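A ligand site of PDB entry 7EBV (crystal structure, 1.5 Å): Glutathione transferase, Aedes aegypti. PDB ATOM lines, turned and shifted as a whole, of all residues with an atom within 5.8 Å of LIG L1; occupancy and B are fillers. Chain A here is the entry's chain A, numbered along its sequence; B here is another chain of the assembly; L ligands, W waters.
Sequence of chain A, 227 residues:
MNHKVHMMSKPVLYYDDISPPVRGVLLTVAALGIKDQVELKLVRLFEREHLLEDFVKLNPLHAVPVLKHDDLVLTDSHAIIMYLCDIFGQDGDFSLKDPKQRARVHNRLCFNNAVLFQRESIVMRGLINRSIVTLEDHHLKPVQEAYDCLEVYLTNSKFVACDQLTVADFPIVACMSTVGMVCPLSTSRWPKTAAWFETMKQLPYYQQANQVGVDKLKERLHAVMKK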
ATOM      1  N   SER A  19     -12.709  -0.266  18.209  1.00  0.00           N
ATOM      2  CA  SER A  19     -11.519  -0.255  19.068  1.00  0.00           C
ATOM      3  C   SER A  19     -11.182   1.166  19.505  1.00  0.00           C
ATOM      4  O   SER A  19     -10.998   2.032  18.653  1.00  0.00           O
ATOM      5  CB  SER A  19     -10.335  -0.821  18.283  1.00  0.00           C
ATOM      6  OG  SER A  19      -9.096  -0.549  18.924  1.00  0.00           O
ATOM      7  N   PRO A  20     -11.010   1.428  20.808  1.00  0.00           N
ATOM      8  CA  PRO A  20     -10.540   2.772  21.231  1.00  0.00           C
ATOM      9  C   PRO A  20      -9.179   3.123  20.645  1.00  0.00           C
ATOM     10  O   PRO A  20      -9.004   4.243  20.150  1.00  0.00           O
ATOM     11  CB  PRO A  20     -10.506   2.676  22.768  1.00  0.00           C
ATOM     12  CG  PRO A  20     -11.413   1.571  23.105  1.00  0.00           C
ATOM     13  CD  PRO A  20     -11.375   0.592  21.954  1.00  0.00           C
ATOM     14  N   PRO A  21      -8.167   2.217  20.654  1.00  0.00           N
ATOM     15  CA  PRO A  21      -6.906   2.581  19.978  1.00  0.00           C
ATOM     16  C   PRO A  21      -7.100   3.029  18.543  1.00  0.00           C
ATOM     17  O   PRO A  21      -6.469   4.000  18.123  1.00  0.00           O
ATOM     18  CB  PRO A  21      -6.084   1.278  20.070  1.00  0.00           C
ATOM     19  CG  PRO A  21      -6.551   0.639  21.319  1.00  0.00           C
ATOM     20  CD  PRO A  21      -8.030   0.955  21.418  1.00  0.00           C
ATOM     21  N   LEU A  45     -12.833  -7.132  13.705  1.00  0.00           N
ATOM     22  CA  LEU A  45     -12.515  -8.002  14.835  1.00  0.00           C
ATOM     23  C   LEU A  45     -13.589  -9.064  15.057  1.00  0.00           C
ATOM     24  O   LEU A  45     -13.279 -10.239  15.299  1.00  0.00           O
ATOM     25  CB  LEU A  45     -12.329  -7.148  16.101  1.00  0.00           C
ATOM     26  CG  LEU A  45     -11.152  -6.161  16.011  1.00  0.00           C
ATOM     27  CD1 LEU A  45     -11.098  -5.331  17.296  1.00  0.00           C
ATOM     28  CD2 LEU A  45      -9.849  -6.907  15.794  1.00  0.00           C
ATOM     29  N   HIS A  50      -8.629 -10.242  11.922  1.00  0.00           N
ATOM     30  CA  HIS A  50      -7.298  -9.998  12.483  1.00  0.00           C
ATOM     31  C   HIS A  50      -6.517 -11.273  12.718  1.00  0.00           C
ATOM     32  O   HIS A  50      -5.341 -11.202  13.096  1.00  0.00           O
ATOM     33  CB  HIS A  50      -7.422  -9.215  13.805  1.00  0.00           C
ATOM     34  CG  HIS A  50      -8.231  -9.926  14.843  1.00  0.00           C
ATOM     35  ND1 HIS A  50      -9.536 -10.316  14.623  1.00  0.00           N
ATOM     36  CD2 HIS A  50      -7.926 -10.307  16.095  1.00  0.00           C
ATOM     37  CE1 HIS A  50      -9.998 -10.900  15.709  1.00  0.00           C
ATOM     38  NE2 HIS A  50      -9.041 -10.911  16.627  1.00  0.00           N
ATOM     39  N   LEU A  51      -7.127 -12.447  12.526  1.00  0.00           N
ATOM     40  CA  LEU A  51      -6.429 -13.700  12.686  1.00  0.00           C
ATOM     41  C   LEU A  51      -6.068 -14.350  11.358  1.00  0.00           C
ATOM     42  O   LEU A  51      -5.480 -15.434  11.352  1.00  0.00           O
ATOM     43  CB  LEU A  51      -7.285 -14.655  13.540  1.00  0.00           C
ATOM     44  CG  LEU A  51      -7.626 -14.082  14.921  1.00  0.00           C
ATOM     45  CD1 LEU A  51      -8.534 -15.057  15.687  1.00  0.00           C
ATOM     46  CD2 LEU A  51      -6.360 -13.790  15.720  1.00  0.00           C
ATOM     47  N   LEU A  61       1.070  -9.405  16.881  1.00  0.00           N
ATOM     48  CA  LEU A  61       0.133  -9.137  17.967  1.00  0.00           C
ATOM     49  C   LEU A  61      -1.318  -9.296  17.536  1.00  0.00           C
ATOM     50  O   LEU A  61      -2.209  -9.254  18.388  1.00  0.00           O
ATOM     51  CB  LEU A  61       0.368  -7.719  18.516  1.00  0.00           C
ATOM     52  CG  LEU A  61       1.738  -7.447  19.149  1.00  0.00           C
ATOM     53  CD1 LEU A  61       2.031  -5.938  19.221  1.00  0.00           C
ATOM     54  CD2 LEU A  61       1.773  -8.098  20.520  1.00  0.00           C
ATOM     55  N   HIS A  62      -1.569  -9.505  16.241  1.00  0.00           N
ATOM     56  CA  HIS A  62      -2.917  -9.711  15.674  1.00  0.00           C
ATOM     57  C   HIS A  62      -3.930  -8.719  16.264  1.00  0.00           C
ATOM     58  O   HIS A  62      -5.019  -9.080  16.734  1.00  0.00           O
ATOM     59  CB  HIS A  62      -3.386 -11.168  15.822  1.00  0.00           C
ATOM     60  CG  HIS A  62      -3.341 -11.719  17.211  1.00  0.00           C
ATOM     61  ND1 HIS A  62      -4.312 -11.456  18.152  1.00  0.00           N
ATOM     62  CD2 HIS A  62      -2.441 -12.535  17.814  1.00  0.00           C
ATOM     63  CE1 HIS A  62      -4.018 -12.096  19.276  1.00  0.00           C
ATOM     64  NE2 HIS A  62      -2.880 -12.744  19.095  1.00  0.00           N
ATOM     65  N   ALA A  63      -3.571  -7.444  16.205  1.00  0.00           N
ATOM     66  CA  ALA A  63      -4.402  -6.392  16.777  1.00  0.00           C
ATOM     67  C   ALA A  63      -4.443  -5.181  15.864  1.00  0.00           C
ATOM     68  O   ALA A  63      -3.551  -4.980  15.020  1.00  0.00           O
ATOM     69  CB  ALA A  63      -3.886  -5.976  18.160  1.00  0.00           C
ATOM     70  N   VAL A  64      -5.486  -4.372  16.020  1.00  0.00           N
ATOM     71  CA  VAL A  64      -5.633  -3.116  15.292  1.00  0.00           C
ATOM     72  C   VAL A  64      -5.507  -1.946  16.259  1.00  0.00           C
ATOM     73  O   VAL A  64      -5.869  -2.073  17.453  1.00  0.00           O
ATOM     74  CB  VAL A  64      -6.961  -3.048  14.525  1.00  0.00           C
ATOM     75  CG1 VAL A  64      -6.942  -4.056  13.347  1.00  0.00           C
ATOM     76  CG2 VAL A  64      -8.150  -3.308  15.468  1.00  0.00           C
ATOM     77  N   PRO A  65      -5.014  -0.782  15.811  1.00  0.00           N
ATOM     78  CA  PRO A  65      -4.620  -0.459  14.433  1.00  0.00           C
ATOM     79  C   PRO A  65      -3.196  -0.843  14.051  1.00  0.00           C
ATOM     80  O   PRO A  65      -2.344  -1.081  14.898  1.00  0.00           O
ATOM     81  CB  PRO A  65      -4.754   1.064  14.390  1.00  0.00           C
ATOM     82  CG  PRO A  65      -4.385   1.485  15.816  1.00  0.00           C
ATOM     83  CD  PRO A  65      -4.927   0.385  16.710  1.00  0.00           C
ATOM     84  N   THR A  75       2.643  -0.866  14.789  1.00  0.00           N
ATOM     85  CA  THR A  75       1.699  -1.815  15.369  1.00  0.00           C
ATOM     86  C   THR A  75       1.256  -1.357  16.747  1.00  0.00           C
ATOM     87  O   THR A  75       0.980  -2.166  17.626  1.00  0.00           O
ATOM     88  CB  THR A  75       2.296  -3.220  15.386  1.00  0.00           C
ATOM     89  OG1 THR A  75       3.539  -3.214  16.115  1.00  0.00           O
ATOM     90  CG2 THR A  75       2.575  -3.696  13.952  1.00  0.00           C
ATOM     91  N   ASP A  76       1.142  -0.054  16.931  1.00  0.00           N
ATOM     92  CA  ASP A  76       0.593   0.512  18.151  1.00  0.00           C
ATOM     93  C   ASP A  76       0.059   1.885  17.807  1.00  0.00           C
ATOM     94  O   ASP A  76       0.760   2.693  17.191  1.00  0.00           O
ATOM     95  CB  ASP A  76       1.623   0.532  19.307  1.00  0.00           C
ATOM     96  CG  ASP A  76       0.993   0.896  20.656  1.00  0.00           C
ATOM     97  OD1 ASP A  76       0.366   1.986  20.750  1.00  0.00           O
ATOM     98  OD2 ASP A  76       0.963   0.022  21.574  1.00  0.00           O
ATOM     99  N   SER A  77      -1.211   2.118  18.193  1.00  0.00           N
ATOM    100  CA  SER A  77      -1.885   3.382  17.884  1.00  0.00           C
ATOM    101  C   SER A  77      -1.074   4.595  18.312  1.00  0.00           C
ATOM    102  O   SER A  77      -1.101   5.623  17.643  1.00  0.00           O
ATOM    103  CB  SER A  77      -3.258   3.419  18.546  1.00  0.00           C
ATOM    104  OG  SER A  77      -3.152   3.470  19.981  1.00  0.00           O
ATOM    105  N   HIS A  78      -0.369   4.486  19.452  1.00  0.00           N
ATOM    106  CA  HIS A  78       0.334   5.664  19.959  1.00  0.00           C
ATOM    107  C   HIS A  78       1.560   5.978  19.107  1.00  0.00           C
ATOM    108  O   HIS A  78       1.879   7.163  18.883  1.00  0.00           O
ATOM    109  CB  HIS A  78       0.656   5.419  21.441  1.00  0.00           C
ATOM    110  CG  HIS A  78      -0.569   5.106  22.243  1.00  0.00           C
ATOM    111  ND1 HIS A  78      -1.074   3.832  22.367  1.00  0.00           N
ATOM    112  CD2 HIS A  78      -1.429   5.918  22.904  1.00  0.00           C
ATOM    113  CE1 HIS A  78      -2.186   3.868  23.097  1.00  0.00           C
ATOM    114  NE2 HIS A  78      -2.430   5.129  23.424  1.00  0.00           N
ATOM    115  N   ASN A 113      -1.753   4.424  26.966  1.00  0.00           N
ATOM    116  CA  ASN A 113      -1.437   3.061  26.536  1.00  0.00           C
ATOM    117  C   ASN A 113      -1.208   2.140  27.728  1.00  0.00           C
ATOM    118  O   ASN A 113      -1.686   0.991  27.733  1.00  0.00           O
ATOM    119  CB  ASN A 113      -0.208   3.075  25.647  1.00  0.00           C
ATOM    120  CG  ASN A 113      -0.173   1.908  24.703  1.00  0.00           C
ATOM    121  OD1 ASN A 113      -1.190   1.234  24.508  1.00  0.00           O
ATOM    122  ND2 ASN A 113       0.964   1.677  24.104  1.00  0.00           N
ATOM    123  N   PHE A 117      -5.967   2.722  28.977  1.00  0.00           N
ATOM    124  CA  PHE A 117      -6.433   1.670  28.071  1.00  0.00           C
ATOM    125  C   PHE A 117      -6.271   0.295  28.686  1.00  0.00           C
ATOM    126  O   PHE A 117      -7.123  -0.580  28.494  1.00  0.00           O
ATOM    127  CB  PHE A 117      -5.693   1.728  26.728  1.00  0.00           C
ATOM    128  CG  PHE A 117      -5.984   0.550  25.825  1.00  0.00           C
ATOM    129  CD1 PHE A 117      -7.243   0.360  25.309  1.00  0.00           C
ATOM    130  CD2 PHE A 117      -4.993  -0.374  25.526  1.00  0.00           C
ATOM    131  CE1 PHE A 117      -7.540  -0.737  24.488  1.00  0.00           C
ATOM    132  CE2 PHE A 117      -5.275  -1.480  24.708  1.00  0.00           C
ATOM    133  CZ  PHE A 117      -6.543  -1.651  24.196  1.00  0.00           C
ATOM    134  N   GLN A 118      -5.171   0.052  29.414  1.00  0.00           N
ATOM    135  CA  GLN A 118      -5.004  -1.260  30.022  1.00  0.00           C
ATOM    136  C   GLN A 118      -6.143  -1.584  30.970  1.00  0.00           C
ATOM    137  O   GLN A 118      -6.668  -2.699  30.973  1.00  0.00           O
ATOM    138  CB  GLN A 118      -3.669  -1.366  30.773  1.00  0.00           C
ATOM    139  CG  GLN A 118      -2.434  -1.265  29.881  1.00  0.00           C
ATOM    140  CD  GLN A 118      -2.447  -2.252  28.726  1.00  0.00           C
ATOM    141  OE1 GLN A 118      -2.821  -3.428  28.872  1.00  0.00           O
ATOM    142  NE2 GLN A 118      -2.042  -1.777  27.553  1.00  0.00           N
ATOM    143  N   CYS B 110       6.460   1.030  22.691  1.00  0.00           N
ATOM    144  CA  CYS B 110       5.055   0.741  22.944  1.00  0.00           C
ATOM    145  C   CYS B 110       4.815  -0.751  23.182  1.00  0.00           C
ATOM    146  O   CYS B 110       4.030  -1.126  24.063  1.00  0.00           O
ATOM    147  CB  CYS B 110       4.205   1.208  21.757  1.00  0.00           C
ATOM    148  SG  CYS B 110       4.106   2.972  21.512  1.00  0.00           S
ATOM    149  N   ALA B 114       3.084  -1.642  26.639  1.00  0.00           N
ATOM    150  CA  ALA B 114       1.694  -2.078  26.559  1.00  0.00           C
ATOM    151  C   ALA B 114       1.523  -3.590  26.477  1.00  0.00           C
ATOM    152  O   ALA B 114       0.393  -4.075  26.658  1.00  0.00           O
ATOM    153  CB  ALA B 114       1.019  -1.432  25.340  1.00  0.00           C
HETATM  154  N1  LIG L   1      -1.507  -0.790  22.590  1.00  0.00           N
HETATM  155  C1  LIG L   1      -2.214  -1.183  21.335  1.00  0.00           C
HETATM  156  C2  LIG L   1      -2.551   0.089  20.543  1.00  0.00           C
HETATM  157  O1  LIG L   1      -2.780   1.105  21.207  1.00  0.00           O
HETATM  158  O2  LIG L   1      -2.568   0.014  19.306  1.00  0.00           O
HETATM  159  C3  LIG L   1      -3.475  -1.982  21.667  1.00  0.00           C
HETATM  160  C4  LIG L   1      -4.170  -2.554  20.434  1.00  0.00           C
HETATM  161  C5  LIG L   1      -5.266  -3.531  20.809  1.00  0.00           C
HETATM  162  O3  LIG L   1      -5.225  -4.184  21.852  1.00  0.00           O
HETATM  163  N2  LIG L   1      -6.283  -3.639  19.949  1.00  0.00           N
HETATM  164  C6  LIG L   1      -7.374  -4.562  20.161  1.00  0.00           C
HETATM  165  C7  LIG L   1      -7.334  -5.764  19.229  1.00  0.00           C
HETATM  166  O4  LIG L   1      -7.218  -5.575  18.017  1.00  0.00           O
HETATM  167  C8  LIG L   1      -8.715  -3.884  20.003  1.00  0.00           C
HETATM  168  S1  LIG L   1      -8.968  -2.574  21.217  1.00  0.00           S
HETATM  169  N3  LIG L   1      -7.423  -6.966  19.806  1.00  0.00           N
HETATM  170  C9  LIG L   1      -7.465  -8.200  19.048  1.00  0.00           C
HETATM  171  C10 LIG L   1      -6.686  -9.321  19.730  1.00  0.00           C
HETATM  172  O5  LIG L   1      -6.071  -9.017  20.771  1.00  0.00           O
HETATM  173  O6  LIG L   1      -6.729 -10.457  19.204  1.00  0.00           O
HETATM  174  C1  LG2 L   2     -13.582  -8.370  19.498  1.00  0.00           C
HETATM  175  O1  LG2 L   2     -14.293 -10.203  18.106  1.00  0.00           O
HETATM  176  C2  LG2 L   2     -13.335  -9.612  18.934  1.00  0.00           C
HETATM  177  O2  LG2 L   2      -9.979 -10.374  20.292  1.00  0.00           O
HETATM  178  C3  LG2 L   2     -12.134 -10.280  19.198  1.00  0.00           C
HETATM  179  O3  LG2 L   2      -9.364  -8.332  21.744  1.00  0.00           O
HETATM  180  C4  LG2 L   2     -11.175  -9.695  20.034  1.00  0.00           C
HETATM  181  O4  LG2 L   2     -12.920  -6.430  20.916  1.00  0.00           O
HETATM  182  C5  LG2 L   2     -11.412  -8.449  20.599  1.00  0.00           C
HETATM  183  O5  LG2 L   2     -10.860  -2.349  25.039  1.00  0.00           O
HETATM  184  C6  LG2 L   2     -12.634  -7.783  20.325  1.00  0.00           C
HETATM  185  O6  LG2 L   2     -12.981  -0.850  24.226  1.00  0.00           O
HETATM  186  C7  LG2 L   2     -10.388  -7.794  21.504  1.00  0.00           C
HETATM  187  C8  LG2 L   2     -10.659  -6.499  22.075  1.00  0.00           C
HETATM  188  C9  LG2 L   2     -11.940  -5.818  21.765  1.00  0.00           C
HETATM  189  C10 LG2 L   2     -12.227  -4.467  22.392  1.00  0.00           C
HETATM  190  C11 LG2 L   2     -11.414  -4.040  23.418  1.00  0.00           C
HETATM  191  C12 LG2 L   2     -11.671  -2.829  24.013  1.00  0.00           C
HETATM  192  C13 LG2 L   2     -12.751  -2.071  23.593  1.00  0.00           C
HETATM  193  C14 LG2 L   2     -13.584  -2.504  22.581  1.00  0.00           C
HETATM  194  C15 LG2 L   2     -13.320  -3.729  21.973  1.00  0.00           C
HETATM  195  O   HOH W   1      -3.855  -4.717  23.969  1.00  0.00           O
HETATM  196  O   HOH W   2      -8.637 -12.285  19.231  1.00  0.00           O
HETATM  197  O   HOH W   3      -2.504  -2.162  17.456  1.00  0.00           O
HETATM  198  O   HOH W   4      -7.798  -4.990  24.050  1.00  0.00           O
HETATM  199  O   HOH W   5      -6.667  -7.088  22.976  1.00  0.00           O
HETATM  200  O   HOH W   6      -1.802  -3.039  24.574  1.00  0.00           O
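Pro 21 touches LIG L1 (CB to O1, 3.5 Å). Leu 45 touches LIG L1 (CD2 to O4, 3.7 Å). CA of Ala 63 touches O4 of LIG L1, 3.2 Å away. Pro 65 touches LIG L1 (CD to O2, 3.5 Å). CE2 of Phe 117 touches C3 of LIG L1 (3.6 Å). Ala 114 of chain B touches LIG L1 (CB to N1, 3.8 Å). Hydrophobic or aromatic side chains that line LIG L1: Pro 21, Leu 45, His 50, His 62, Ala 63, Val 64, Pro 65, His 78, Phe 117 and Ala 114 of chain B. Of the 20 residues printed, 14 come within 4 Å of LIG L1. Along chain A the residues within 4 Å of LIG L1 span positions 19 to 117.
Water W2 lies within hydrogen-bond range of O2 of LG2 L2 (2.6 Å), O6 of LIG L1 (2.6 Å) and NE2 of His 50 (3.0 Å). Water W5 lies within hydrogen-bond range of O5 of LIG L1 (3.0 Å) and O3 of LG2 L2 (3.2 Å). Water W6 lies within hydrogen-bond range of a nitrogen (N1) of LIG L1 (3.0 Å), the backbone carbonyl oxygen (O) of Ala 114 of chain B (3.2 Å) and the side-chain amide nitrogen (NE2) of Gln 118 (3.2 Å).
An oxygen (O3) of LG2 L2 sits at hydrogen-bond distance from a nitrogen (N3) of LIG L1 (3.1 Å).
A ring nitrogen (ND1) of His 78 sits at hydrogen-bond distance from the side-chain hydroxyl of Ser 77 (3.2 Å). OD2 of Asp 76 is in hydrogen-bond range of ND2 of Asn 113 (3.0 Å). ND1 of His 78 sits at hydrogen-bond distance from OD1 of Asp 76, 2.8 Å away. A ring nitrogen (ND1) of His 78 sits close to the side-chain amide oxygen of Asn 113 (3.4 Å). The backbone carbonyl oxygen of Asn 113 is in hydrogen-bond range of the side-chain amide nitrogen of Gln 118, at 2.8 Å. NE2 of Gln 118 is in hydrogen-bond range of O of Ala 114 of chain B.
The backbone NH (N) of Ser 77 is in hydrogen-bond range of an oxygen (O2) of LIG L1. The side-chain hydroxyl (OG) of Ser 77 is in hydrogen-bond range of an oxygen (O1) of LIG L1 (2.7 Å). The side-chain carboxylate (OD2) of Asp 76 lies within salt-bridge range of a nitrogen (N1) of LIG L1 (2.8 Å). A nitrogen (N1) of LIG L1 sits at hydrogen-bond distance from the side-chain amide oxygen (OD1) of Asn 113. An oxygen (O6) of LIG L1 lies within hydrogen-bond range of a ring nitrogen (ND1) of His 62, 2.8 Å away. The backbone NH (N) of Val 64 is in hydrogen-bond range of an oxygen (O4) of LIG L1, at 2.9 Å. The backbone carbonyl oxygen (O) of Val 64 sits at hydrogen-bond distance from a nitrogen (N2) of LIG L1, at 3.0 Å. S1 of LIG L1 lies close to OG of Ser 19, 3.1 Å away. NE2 of His 50 lies close to O6 of LIG L1 (3.5 Å). ND1 of His 78 sits close to O1 of LIG L1 (3.4 Å). The backbone carbonyl oxygen (O) of Leu 45 is in hydrogen-bond range of an oxygen (O1) of LG2 L2 (3.0 Å).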
